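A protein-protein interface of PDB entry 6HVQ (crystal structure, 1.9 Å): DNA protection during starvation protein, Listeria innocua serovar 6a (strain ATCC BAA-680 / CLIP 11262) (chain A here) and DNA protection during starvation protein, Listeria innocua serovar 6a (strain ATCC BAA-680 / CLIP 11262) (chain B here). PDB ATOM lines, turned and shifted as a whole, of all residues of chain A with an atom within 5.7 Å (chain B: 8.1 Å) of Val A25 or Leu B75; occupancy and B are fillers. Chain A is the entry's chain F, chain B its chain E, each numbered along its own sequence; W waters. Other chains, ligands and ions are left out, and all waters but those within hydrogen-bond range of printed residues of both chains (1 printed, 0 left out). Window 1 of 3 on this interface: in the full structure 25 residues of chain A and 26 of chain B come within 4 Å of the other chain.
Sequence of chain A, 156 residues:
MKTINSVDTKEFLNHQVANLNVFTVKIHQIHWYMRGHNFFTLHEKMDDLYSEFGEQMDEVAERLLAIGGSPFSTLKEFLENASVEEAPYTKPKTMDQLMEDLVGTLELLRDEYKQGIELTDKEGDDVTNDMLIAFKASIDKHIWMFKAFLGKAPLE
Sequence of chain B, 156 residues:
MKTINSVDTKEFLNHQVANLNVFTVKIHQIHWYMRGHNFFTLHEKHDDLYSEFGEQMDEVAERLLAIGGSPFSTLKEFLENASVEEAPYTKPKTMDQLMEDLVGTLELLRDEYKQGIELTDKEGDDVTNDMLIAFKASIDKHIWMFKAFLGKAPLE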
ATOM      1  N   LEU A  20      -4.785  27.518  11.681  1.00  0.00           N
ATOM      2  CA  LEU A  20      -5.068  28.454  12.758  1.00  0.00           C
ATOM      3  C   LEU A  20      -4.691  27.882  14.114  1.00  0.00           C
ATOM      4  O   LEU A  20      -4.278  28.641  15.003  1.00  0.00           O
ATOM      5  CB  LEU A  20      -6.543  28.849  12.729  1.00  0.00           C
ATOM      6  CG  LEU A  20      -6.913  29.787  11.591  1.00  0.00           C
ATOM      7  CD1 LEU A  20      -8.416  29.841  11.394  1.00  0.00           C
ATOM      8  CD2 LEU A  20      -6.382  31.181  11.900  1.00  0.00           C
ATOM      9  N   ASN A  21      -4.797  26.562  14.306  1.00  0.00           N
ATOM     10  CA  ASN A  21      -4.309  26.005  15.570  1.00  0.00           C
ATOM     11  C   ASN A  21      -2.785  26.108  15.681  1.00  0.00           C
ATOM     12  O   ASN A  21      -2.250  26.509  16.738  1.00  0.00           O
ATOM     13  CB  ASN A  21      -4.780  24.563  15.725  1.00  0.00           C
ATOM     14  CG  ASN A  21      -6.175  24.478  16.331  1.00  0.00           C
ATOM     15  OD1 ASN A  21      -6.332  24.493  17.548  1.00  0.00           O
ATOM     16  ND2 ASN A  21      -7.192  24.405  15.479  1.00  0.00           N
ATOM     17  N   VAL A  22      -2.062  25.805  14.593  1.00  0.00           N
ATOM     18  CA  VAL A  22      -0.608  25.994  14.634  1.00  0.00           C
ATOM     19  C   VAL A  22      -0.272  27.455  14.922  1.00  0.00           C
ATOM     20  O   VAL A  22       0.624  27.765  15.724  1.00  0.00           O
ATOM     21  CB  VAL A  22       0.042  25.520  13.320  1.00  0.00           C
ATOM     22  CG1 VAL A  22       1.554  25.735  13.363  1.00  0.00           C
ATOM     23  CG2 VAL A  22      -0.276  24.054  13.051  1.00  0.00           C
ATOM     24  N   PHE A  23      -1.007  28.375  14.293  1.00  0.00           N
ATOM     25  CA  PHE A  23      -0.718  29.796  14.434  1.00  0.00           C
ATOM     26  C   PHE A  23      -0.950  30.273  15.859  1.00  0.00           C
ATOM     27  O   PHE A  23      -0.155  31.058  16.388  1.00  0.00           O
ATOM     28  CB  PHE A  23      -1.570  30.604  13.453  1.00  0.00           C
ATOM     29  CG  PHE A  23      -1.246  32.076  13.415  1.00  0.00           C
ATOM     30  CD1 PHE A  23       0.042  32.537  13.644  1.00  0.00           C
ATOM     31  CD2 PHE A  23      -2.239  33.001  13.128  1.00  0.00           C
ATOM     32  CE1 PHE A  23       0.328  33.892  13.594  1.00  0.00           C
ATOM     33  CE2 PHE A  23      -1.961  34.354  13.073  1.00  0.00           C
ATOM     34  CZ  PHE A  23      -0.673  34.802  13.312  1.00  0.00           C
ATOM     35  N   THR A  24      -2.042  29.843  16.499  1.00  0.00           N
ATOM     36  CA  THR A  24      -2.266  30.313  17.862  1.00  0.00           C
ATOM     37  C   THR A  24      -1.168  29.811  18.794  1.00  0.00           C
ATOM     38  O   THR A  24      -0.693  30.560  19.663  1.00  0.00           O
ATOM     39  CB  THR A  24      -3.644  29.893  18.374  1.00  0.00           C
ATOM     40  OG1 THR A  24      -3.826  28.496  18.172  1.00  0.00           O
ATOM     41  CG2 THR A  24      -4.751  30.668  17.658  1.00  0.00           C
ATOM     42  N   VAL A  25      -0.707  28.569  18.598  1.00  0.00           N
ATOM     43  CA  VAL A  25       0.414  28.104  19.417  1.00  0.00           C
ATOM     44  C   VAL A  25       1.659  28.962  19.166  1.00  0.00           C
ATOM     45  O   VAL A  25       2.424  29.266  20.098  1.00  0.00           O
ATOM     46  CB  VAL A  25       0.669  26.605  19.174  1.00  0.00           C
ATOM     47  CG1 VAL A  25       1.950  26.141  19.857  1.00  0.00           C
ATOM     48  CG2 VAL A  25      -0.514  25.793  19.699  1.00  0.00           C
ATOM     49  N   LYS A  26       1.888  29.371  17.909  1.00  0.00           N
ATOM     50  CA  LYS A  26       3.016  30.264  17.633  1.00  0.00           C
ATOM     51  C   LYS A  26       2.853  31.606  18.351  1.00  0.00           C
ATOM     52  O   LYS A  26       3.823  32.157  18.893  1.00  0.00           O
ATOM     53  CB  LYS A  26       3.168  30.473  16.125  1.00  0.00           C
ATOM     54  CG  LYS A  26       4.353  31.357  15.729  1.00  0.00           C
ATOM     55  CD  LYS A  26       4.351  31.696  14.237  1.00  0.00           C
ATOM     56  CE  LYS A  26       4.637  30.476  13.369  1.00  0.00           C
ATOM     57  NZ  LYS A  26       6.045  29.992  13.486  1.00  0.00           N
ATOM     58  N   ILE A  27       1.629  32.142  18.374  1.00  0.00           N
ATOM     59  CA  ILE A  27       1.390  33.404  19.063  1.00  0.00           C
ATOM     60  C   ILE A  27       1.758  33.272  20.533  1.00  0.00           C
ATOM     61  O   ILE A  27       2.362  34.179  21.117  1.00  0.00           O
ATOM     62  CB  ILE A  27      -0.073  33.855  18.867  1.00  0.00           C
ATOM     63  CG1 ILE A  27      -0.309  34.238  17.405  1.00  0.00           C
ATOM     64  CG2 ILE A  27      -0.427  35.016  19.797  1.00  0.00           C
ATOM     65  CD1 ILE A  27      -1.770  34.414  17.035  1.00  0.00           C
ATOM     66  N   HIS A  28       1.423  32.136  21.154  1.00  0.00           N
ATOM     67  CA  HIS A  28       1.833  31.929  22.545  1.00  0.00           C
ATOM     68  C   HIS A  28       3.350  31.815  22.688  1.00  0.00           C
ATOM     69  O   HIS A  28       3.920  32.337  23.656  1.00  0.00           O
ATOM     70  CB  HIS A  28       1.148  30.692  23.123  1.00  0.00           C
ATOM     71  CG  HIS A  28      -0.053  30.998  23.968  1.00  0.00           C
ATOM     72  ND1 HIS A  28      -0.817  30.009  24.550  1.00  0.00           N
ATOM     73  CD2 HIS A  28      -0.615  32.174  24.337  1.00  0.00           C
ATOM     74  CE1 HIS A  28      -1.801  30.562  25.238  1.00  0.00           C
ATOM     75  NE2 HIS A  28      -1.704  31.874  25.122  1.00  0.00           N
ATOM     76  N   GLN A  29       4.025  31.119  21.761  1.00  0.00           N
ATOM     77  CA  GLN A  29       5.490  31.073  21.793  1.00  0.00           C
ATOM     78  C   GLN A  29       6.086  32.479  21.845  1.00  0.00           C
ATOM     79  O   GLN A  29       6.974  32.774  22.662  1.00  0.00           O
ATOM     80  CB  GLN A  29       6.018  30.318  20.564  1.00  0.00           C
ATOM     81  CG  GLN A  29       7.548  30.234  20.448  1.00  0.00           C
ATOM     82  CD  GLN A  29       8.009  29.516  19.179  1.00  0.00           C
ATOM     83  OE1 GLN A  29       8.218  30.143  18.139  1.00  0.00           O
ATOM     84  NE2 GLN A  29       8.163  28.199  19.259  1.00  0.00           N
ATOM     85  N   ILE A  30       5.619  33.357  20.955  1.00  0.00           N
ATOM     86  CA  ILE A  30       6.136  34.723  20.915  1.00  0.00           C
ATOM     87  C   ILE A  30       5.805  35.453  22.209  1.00  0.00           C
ATOM     88  O   ILE A  30       6.646  36.164  22.777  1.00  0.00           O
ATOM     89  CB  ILE A  30       5.576  35.460  19.683  1.00  0.00           C
ATOM     90  CG1 ILE A  30       6.073  34.793  18.390  1.00  0.00           C
ATOM     91  CG2 ILE A  30       5.966  36.926  19.725  1.00  0.00           C
ATOM     92  CD1 ILE A  30       5.380  35.288  17.130  1.00  0.00           C
ATOM     93  N   TYR A  50      -4.067  36.241  19.955  1.00  0.00           N
ATOM     94  CA  TYR A  50      -4.447  34.892  20.348  1.00  0.00           C
ATOM     95  C   TYR A  50      -5.961  34.760  20.399  1.00  0.00           C
ATOM     96  O   TYR A  50      -6.535  33.824  19.825  1.00  0.00           O
ATOM     97  CB  TYR A  50      -3.818  34.549  21.700  1.00  0.00           C
ATOM     98  CG  TYR A  50      -3.969  33.098  22.088  1.00  0.00           C
ATOM     99  CD1 TYR A  50      -3.076  32.146  21.612  1.00  0.00           C
ATOM    100  CD2 TYR A  50      -4.992  32.677  22.930  1.00  0.00           C
ATOM    101  CE1 TYR A  50      -3.195  30.815  21.955  1.00  0.00           C
ATOM    102  CE2 TYR A  50      -5.120  31.338  23.285  1.00  0.00           C
ATOM    103  CZ  TYR A  50      -4.215  30.413  22.789  1.00  0.00           C
ATOM    104  OH  TYR A  50      -4.321  29.080  23.122  1.00  0.00           O
ATOM    105  N   LEU A  75      -4.294  17.386  17.762  1.00  0.00           N
ATOM    106  CA  LEU A  75      -2.998  17.950  17.395  1.00  0.00           C
ATOM    107  C   LEU A  75      -2.366  17.170  16.249  1.00  0.00           C
ATOM    108  O   LEU A  75      -1.716  17.751  15.375  1.00  0.00           O
ATOM    109  CB  LEU A  75      -2.059  17.965  18.604  1.00  0.00           C
ATOM    110  CG  LEU A  75      -2.256  19.081  19.628  1.00  0.00           C
ATOM    111  CD1 LEU A  75      -3.588  18.959  20.326  1.00  0.00           C
ATOM    112  CD2 LEU A  75      -1.124  19.050  20.647  1.00  0.00           C
ATOM    113  N   PHE A  78      -3.784  18.447  13.069  1.00  0.00           N
ATOM    114  CA  PHE A  78      -3.306  19.797  12.772  1.00  0.00           C
ATOM    115  C   PHE A  78      -1.893  19.756  12.206  1.00  0.00           C
ATOM    116  O   PHE A  78      -1.598  20.405  11.194  1.00  0.00           O
ATOM    117  CB  PHE A  78      -3.341  20.682  14.018  1.00  0.00           C
ATOM    118  CG  PHE A  78      -4.700  20.805  14.658  1.00  0.00           C
ATOM    119  CD1 PHE A  78      -5.864  20.603  13.931  1.00  0.00           C
ATOM    120  CD2 PHE A  78      -4.802  21.143  15.997  1.00  0.00           C
ATOM    121  CE1 PHE A  78      -7.100  20.720  14.533  1.00  0.00           C
ATOM    122  CE2 PHE A  78      -6.030  21.262  16.605  1.00  0.00           C
ATOM    123  CZ  PHE A  78      -7.185  21.051  15.875  1.00  0.00           C
ATOM    124  N   LEU A  79      -0.997  19.006  12.852  1.00  0.00           N
ATOM    125  CA  LEU A  79       0.367  18.906  12.339  1.00  0.00           C
ATOM    126  C   LEU A  79       0.390  18.250  10.972  1.00  0.00           C
ATOM    127  O   LEU A  79       1.143  18.669  10.086  1.00  0.00           O
ATOM    128  CB  LEU A  79       1.260  18.114  13.293  1.00  0.00           C
ATOM    129  CG  LEU A  79       2.020  18.869  14.371  1.00  0.00           C
ATOM    130  CD1 LEU A  79       2.755  17.883  15.252  1.00  0.00           C
ATOM    131  CD2 LEU A  79       3.004  19.831  13.726  1.00  0.00           C
ATOM    132  N   GLU A  86       6.170  25.750  12.209  1.00  0.00           N
ATOM    133  CA  GLU A  86       6.551  25.964  13.596  1.00  0.00           C
ATOM    134  C   GLU A  86       7.959  25.427  13.805  1.00  0.00           C
ATOM    135  O   GLU A  86       8.421  24.541  13.080  1.00  0.00           O
ATOM    136  CB  GLU A  86       5.578  25.273  14.564  1.00  0.00           C
ATOM    137  CG  GLU A  86       5.476  23.763  14.354  1.00  0.00           C
ATOM    138  CD  GLU A  86       4.717  23.054  15.468  1.00  0.00           C
ATOM    139  OE1 GLU A  86       3.893  23.708  16.154  1.00  0.00           O
ATOM    140  OE2 GLU A  86       4.973  21.844  15.679  1.00  0.00           O
ATOM    141  N   ALA B  18       2.268  20.691  28.004  1.00  0.00           N
ATOM    142  CA  ALA B  18       1.904  19.782  26.915  1.00  0.00           C
ATOM    143  C   ALA B  18       0.506  19.195  27.131  1.00  0.00           C
ATOM    144  O   ALA B  18      -0.355  19.233  26.229  1.00  0.00           O
ATOM    145  CB  ALA B  18       2.958  18.677  26.785  1.00  0.00           C
ATOM    146  N   ASN B  21      -2.404  21.713  26.526  1.00  0.00           N
ATOM    147  CA  ASN B  21      -2.702  21.996  25.121  1.00  0.00           C
ATOM    148  C   ASN B  21      -3.481  20.848  24.471  1.00  0.00           C
ATOM    149  O   ASN B  21      -4.480  21.080  23.756  1.00  0.00           O
ATOM    150  CB  ASN B  21      -1.410  22.292  24.366  1.00  0.00           C
ATOM    151  CG  ASN B  21      -0.997  23.747  24.482  1.00  0.00           C
ATOM    152  OD1 ASN B  21      -1.450  24.593  23.709  1.00  0.00           O
ATOM    153  ND2 ASN B  21      -0.146  24.050  25.458  1.00  0.00           N
ATOM    154  N   VAL B  22      -3.085  19.597  24.746  1.00  0.00           N
ATOM    155  CA  VAL B  22      -3.888  18.476  24.246  1.00  0.00           C
ATOM    156  C   VAL B  22      -5.317  18.555  24.780  1.00  0.00           C
ATOM    157  O   VAL B  22      -6.289  18.293  24.053  1.00  0.00           O
ATOM    158  CB  VAL B  22      -3.226  17.128  24.593  1.00  0.00           C
ATOM    159  CG1 VAL B  22      -4.109  15.968  24.169  1.00  0.00           C
ATOM    160  CG2 VAL B  22      -1.887  17.004  23.879  1.00  0.00           C
ATOM    161  N   THR B  24      -7.182  21.208  25.863  1.00  0.00           N
ATOM    162  CA  THR B  24      -8.033  22.252  25.301  1.00  0.00           C
ATOM    163  C   THR B  24      -8.480  21.879  23.889  1.00  0.00           C
ATOM    164  O   THR B  24      -9.632  22.140  23.498  1.00  0.00           O
ATOM    165  CB  THR B  24      -7.311  23.603  25.309  1.00  0.00           C
ATOM    166  OG1 THR B  24      -6.018  23.474  24.710  1.00  0.00           O
ATOM    167  CG2 THR B  24      -7.153  24.126  26.736  1.00  0.00           C
ATOM    168  N   VAL B  25      -7.598  21.249  23.109  1.00  0.00           N
ATOM    169  CA  VAL B  25      -8.054  20.788  21.795  1.00  0.00           C
ATOM    170  C   VAL B  25      -9.146  19.720  21.940  1.00  0.00           C
ATOM    171  O   VAL B  25     -10.129  19.710  21.184  1.00  0.00           O
ATOM    172  CB  VAL B  25      -6.862  20.312  20.948  1.00  0.00           C
ATOM    173  CG1 VAL B  25      -7.333  19.670  19.642  1.00  0.00           C
ATOM    174  CG2 VAL B  25      -5.955  21.501  20.652  1.00  0.00           C
ATOM    175  N   MET B  57      -3.117  26.817  31.444  1.00  0.00           N
ATOM    176  CA  MET B  57      -1.942  26.515  30.637  1.00  0.00           C
ATOM    177  C   MET B  57      -0.995  27.711  30.581  1.00  0.00           C
ATOM    178  O   MET B  57       0.219  27.567  30.785  1.00  0.00           O
ATOM    179  CB  MET B  57      -2.386  26.089  29.242  1.00  0.00           C
ATOM    180  CG  MET B  57      -1.274  25.554  28.391  1.00  0.00           C
ATOM    181  SD  MET B  57      -0.512  26.879  27.450  1.00  0.00           S
ATOM    182  CE  MET B  57      -1.793  27.145  26.231  1.00  0.00           C
ATOM    183  N   PHE B  72       7.585  24.196  26.539  1.00  0.00           N
ATOM    184  CA  PHE B  72       7.233  23.703  25.218  1.00  0.00           C
ATOM    185  C   PHE B  72       6.324  24.721  24.545  1.00  0.00           C
ATOM    186  O   PHE B  72       5.512  25.372  25.204  1.00  0.00           O
ATOM    187  CB  PHE B  72       6.514  22.355  25.326  1.00  0.00           C
ATOM    188  CG  PHE B  72       7.322  21.263  25.986  1.00  0.00           C
ATOM    189  CD1 PHE B  72       8.624  20.994  25.604  1.00  0.00           C
ATOM    190  CD2 PHE B  72       6.754  20.492  26.983  1.00  0.00           C
ATOM    191  CE1 PHE B  72       9.346  19.977  26.213  1.00  0.00           C
ATOM    192  CE2 PHE B  72       7.464  19.476  27.594  1.00  0.00           C
ATOM    193  CZ  PHE B  72       8.759  19.216  27.212  1.00  0.00           C
ATOM    194  N   SER B  73       6.483  24.888  23.223  1.00  0.00           N
ATOM    195  CA  SER B  73       5.714  25.910  22.522  1.00  0.00           C
ATOM    196  C   SER B  73       5.496  25.559  21.058  1.00  0.00           C
ATOM    197  O   SER B  73       5.386  26.458  20.214  1.00  0.00           O
ATOM    198  CB  SER B  73       6.400  27.269  22.624  1.00  0.00           C
ATOM    199  OG  SER B  73       7.668  27.238  22.000  1.00  0.00           O
ATOM    200  N   THR B  74       5.419  24.267  20.747  1.00  0.00           N
ATOM    201  CA  THR B  74       5.075  23.769  19.421  1.00  0.00           C
ATOM    202  C   THR B  74       4.169  22.560  19.593  1.00  0.00           C
ATOM    203  O   THR B  74       4.223  21.869  20.616  1.00  0.00           O
ATOM    204  CB  THR B  74       6.302  23.339  18.594  1.00  0.00           C
ATOM    205  OG1 THR B  74       7.012  22.311  19.290  1.00  0.00           O
ATOM    206  CG2 THR B  74       7.241  24.501  18.302  1.00  0.00           C
ATOM    207  N   LEU B  75       3.337  22.299  18.585  1.00  0.00           N
ATOM    208  CA  LEU B  75       2.494  21.108  18.634  1.00  0.00           C
ATOM    209  C   LEU B  75       3.338  19.845  18.698  1.00  0.00           C
ATOM    210  O   LEU B  75       2.990  18.891  19.402  1.00  0.00           O
ATOM    211  CB  LEU B  75       1.558  21.065  17.427  1.00  0.00           C
ATOM    212  CG  LEU B  75       0.317  21.953  17.505  1.00  0.00           C
ATOM    213  CD1 LEU B  75       0.693  23.420  17.512  1.00  0.00           C
ATOM    214  CD2 LEU B  75      -0.616  21.645  16.348  1.00  0.00           C
ATOM    215  N   LYS B  76       4.451  19.819  17.964  1.00  0.00           N
ATOM    216  CA  LYS B  76       5.327  18.654  17.979  1.00  0.00           C
ATOM    217  C   LYS B  76       5.783  18.330  19.398  1.00  0.00           C
ATOM    218  O   LYS B  76       5.752  17.169  19.831  1.00  0.00           O
ATOM    219  CB  LYS B  76       6.527  18.910  17.064  1.00  0.00           C
ATOM    220  CG  LYS B  76       7.471  17.729  16.906  1.00  0.00           C
ATOM    221  CD  LYS B  76       8.608  18.065  15.947  1.00  0.00           C
ATOM    222  CE  LYS B  76       9.597  16.919  15.813  1.00  0.00           C
ATOM    223  NZ  LYS B  76      10.693  17.249  14.862  1.00  0.00           N
ATOM    224  N   GLU B  77       6.215  19.348  20.138  1.00  0.00           N
ATOM    225  CA  GLU B  77       6.625  19.140  21.524  1.00  0.00           C
ATOM    226  C   GLU B  77       5.455  18.668  22.392  1.00  0.00           C
ATOM    227  O   GLU B  77       5.611  17.754  23.217  1.00  0.00           O
ATOM    228  CB  GLU B  77       7.226  20.434  22.077  1.00  0.00           C
ATOM    229  CG  GLU B  77       8.614  20.756  21.527  1.00  0.00           C
ATOM    230  CD  GLU B  77       9.107  22.135  21.944  1.00  0.00           C
ATOM    231  OE1 GLU B  77       8.424  23.140  21.643  1.00  0.00           O
ATOM    232  OE2 GLU B  77      10.174  22.213  22.581  1.00  0.00           O
ATOM    233  N   PHE B  78       4.273  19.274  22.224  1.00  0.00           N
ATOM    234  CA  PHE B  78       3.126  18.858  23.029  1.00  0.00           C
ATOM    235  C   PHE B  78       2.823  17.381  22.801  1.00  0.00           C
ATOM    236  O   PHE B  78       2.672  16.608  23.756  1.00  0.00           O
ATOM    237  CB  PHE B  78       1.885  19.695  22.704  1.00  0.00           C
ATOM    238  CG  PHE B  78       2.055  21.173  22.894  1.00  0.00           C
ATOM    239  CD1 PHE B  78       3.004  21.690  23.763  1.00  0.00           C
ATOM    240  CD2 PHE B  78       1.237  22.052  22.204  1.00  0.00           C
ATOM    241  CE1 PHE B  78       3.140  23.067  23.922  1.00  0.00           C
ATOM    242  CE2 PHE B  78       1.368  23.421  22.358  1.00  0.00           C
ATOM    243  CZ  PHE B  78       2.321  23.926  23.221  1.00  0.00           C
ATOM    244  N   LEU B  79       2.759  16.965  21.533  1.00  0.00           N
ATOM    245  CA  LEU B  79       2.457  15.571  21.227  1.00  0.00           C
ATOM    246  C   LEU B  79       3.539  14.640  21.744  1.00  0.00           C
ATOM    247  O   LEU B  79       3.239  13.564  22.272  1.00  0.00           O
ATOM    248  CB  LEU B  79       2.284  15.375  19.723  1.00  0.00           C
ATOM    249  CG  LEU B  79       0.882  15.546  19.154  1.00  0.00           C
ATOM    250  CD1 LEU B  79       0.926  15.433  17.647  1.00  0.00           C
ATOM    251  CD2 LEU B  79      -0.049  14.489  19.732  1.00  0.00           C
ATOM    252  N   GLU B  80       4.806  15.025  21.594  1.00  0.00           N
ATOM    253  CA  GLU B  80       5.877  14.145  22.043  1.00  0.00           C
ATOM    254  C   GLU B  80       5.859  13.969  23.556  1.00  0.00           C
ATOM    255  O   GLU B  80       6.304  12.930  24.052  1.00  0.00           O
ATOM    256  CB  GLU B  80       7.234  14.680  21.582  1.00  0.00           C
ATOM    257  CG  GLU B  80       8.436  13.792  21.935  1.00  0.00           C
ATOM    258  CD  GLU B  80       8.620  12.620  20.984  1.00  0.00           C
ATOM    259  OE1 GLU B  80       7.631  11.909  20.706  1.00  0.00           O
ATOM    260  OE2 GLU B  80       9.757  12.412  20.509  1.00  0.00           O
ATOM    261  N   ASN B  81       5.337  14.944  24.308  1.00  0.00           N
ATOM    262  CA  ASN B  81       5.489  14.910  25.759  1.00  0.00           C
ATOM    263  C   ASN B  81       4.218  14.664  26.565  1.00  0.00           C
ATOM    264  O   ASN B  81       4.329  14.222  27.710  1.00  0.00           O
ATOM    265  CB  ASN B  81       6.093  16.236  26.250  1.00  0.00           C
ATOM    266  CG  ASN B  81       7.556  16.370  25.905  1.00  0.00           C
ATOM    267  OD1 ASN B  81       8.414  15.868  26.624  1.00  0.00           O
ATOM    268  ND2 ASN B  81       7.850  17.056  24.812  1.00  0.00           N
ATOM    269  N   ALA B  82       3.028  14.913  26.019  1.00  0.00           N
ATOM    270  CA  ALA B  82       1.823  14.853  26.838  1.00  0.00           C
ATOM    271  C   ALA B  82       1.466  13.415  27.192  1.00  0.00           C
ATOM    272  O   ALA B  82       1.662  12.489  26.395  1.00  0.00           O
ATOM    273  CB  ALA B  82       0.651  15.532  26.127  1.00  0.00           C
ATOM    274  N   GLU B  86      -5.396  11.710  22.886  1.00  0.00           N
ATOM    275  CA  GLU B  86      -6.364  12.251  21.947  1.00  0.00           C
ATOM    276  C   GLU B  86      -6.621  11.209  20.864  1.00  0.00           C
ATOM    277  O   GLU B  86      -5.792  10.330  20.608  1.00  0.00           O
ATOM    278  CB  GLU B  86      -5.876  13.570  21.319  1.00  0.00           C
ATOM    279  CG  GLU B  86      -4.549  13.442  20.566  1.00  0.00           C
ATOM    280  CD  GLU B  86      -4.200  14.677  19.738  1.00  0.00           C
ATOM    281  OE1 GLU B  86      -4.700  15.785  20.040  1.00  0.00           O
ATOM    282  OE2 GLU B  86      -3.426  14.529  18.764  1.00  0.00           O
HETATM  283  O   HOH W   1      -0.283  27.262  23.382  1.00  0.00           O
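NE2 of Gln A29 is in hydrogen-bond range of OG of Ser B73 (2.9 Å).
OE1 of Glu B86 lies within hydrogen-bond range of N of Leu A75, at 2.8 Å.
N of Leu B75 lies within hydrogen-bond range of OE1 of Glu A86.
The side-chain carboxylate (OE2) of Glu A86 is in hydrogen-bond range of the backbone NH (N) of Lys B76, at 3.1 Å.
The side-chain amide nitrogen (ND2) of Asn B21 lies within hydrogen-bond range of the side-chain sulfur (SD) of Met B57.
The side-chain carboxylate of Glu B77 sits at hydrogen-bond distance from the backbone NH of Ser B73 (3.1 Å).
The side-chain hydroxyl of Thr B74 lies within hydrogen-bond range of the side-chain carboxylate of Glu B77 (2.9 Å).
Among the printed residues, pairs that only touch across the chains: Val A25 with Ser B73 (3.5 Å), Val A25 with Thr B74 (3.9 Å), Val A25 with Leu B75 (3.4 Å), Val A25 with Phe B78 (3.7 Å), His A28 with Met B57 (3.5 Å), Gln A29 with Thr B74 (3.9 Å), Leu A75 with Val B22 (3.9 Å), Leu A75 with Val B25 (3.5 Å), Leu A75 with Phe B78 (3.7 Å), Leu A75 with Leu B79 (3.8 Å), Phe A78 with Val B25 (3.7 Å), Phe A78 with Leu B75 (3.7 Å), Leu A79 with Leu B75 (3.8 Å), Leu A79 with Lys B76 (3.7 Å), Leu A79 with Leu B79 (3.9 Å) and Glu A86 with Thr B74 (3.4 Å).
Of chain A, only Val A25 (3.4 Å), Phe A78 (3.7 Å), Leu A79 (3.8 Å) and Glu A86 (2.9 Å) come within 4 Å of Leu B75.
Of the printed residues of chain A, Thr B74 touches Val A25 (3.9 Å), Gln A29 (3.9 Å) and Glu A86 (3.4 Å).
Printed residues of chain A within 4 Å of Glu B86: Leu A75 (2.8 Å).
Of the printed residues of chain B, Gln A29 touches Ser B73 and Thr B74.
Printed residues of chain A within 4 Å of Leu B79: Leu A75 and Leu A79.
Of the printed residues of chain B, Glu A86 touches Thr B74 (3.4 Å), Leu B75 (2.9 Å) and Lys B76 (3.1 Å).
The nearest residue of chain B that does not touch Val A25 is Asn B21 (4.3 Å).
Of the 18 printed residues of chain B, 10 touch a printed residue of chain A.
Printed residues of chain B that touch a printed residue of chain A: Val B22, Val B25, Met B57, Ser B73, Thr B74, Leu B75, Lys B76, Phe B78, Leu B79 and Glu B86.
Hydrophobic or aromatic side chains of chain B within 4 Å of the printed part of chain A: Val B22, Val B25, Met B57, Leu B75, Phe B78 and Leu B79.
Printed residues of chain A that touch a printed residue of chain B: Val A25, His A28, Gln A29, Leu A75, Phe A78, Leu A79 and Glu A86.
Among the printed residues, 20 pairs touch across the chains.
Among the printed residues, no Asp or Glu carboxylate lies within 4 Å of a Lys or Arg side-chain nitrogen of the other chain.
Water W1 bridges the side-chain amide oxygen of Asn B21 and a ring nitrogen (ND1) of His A28.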
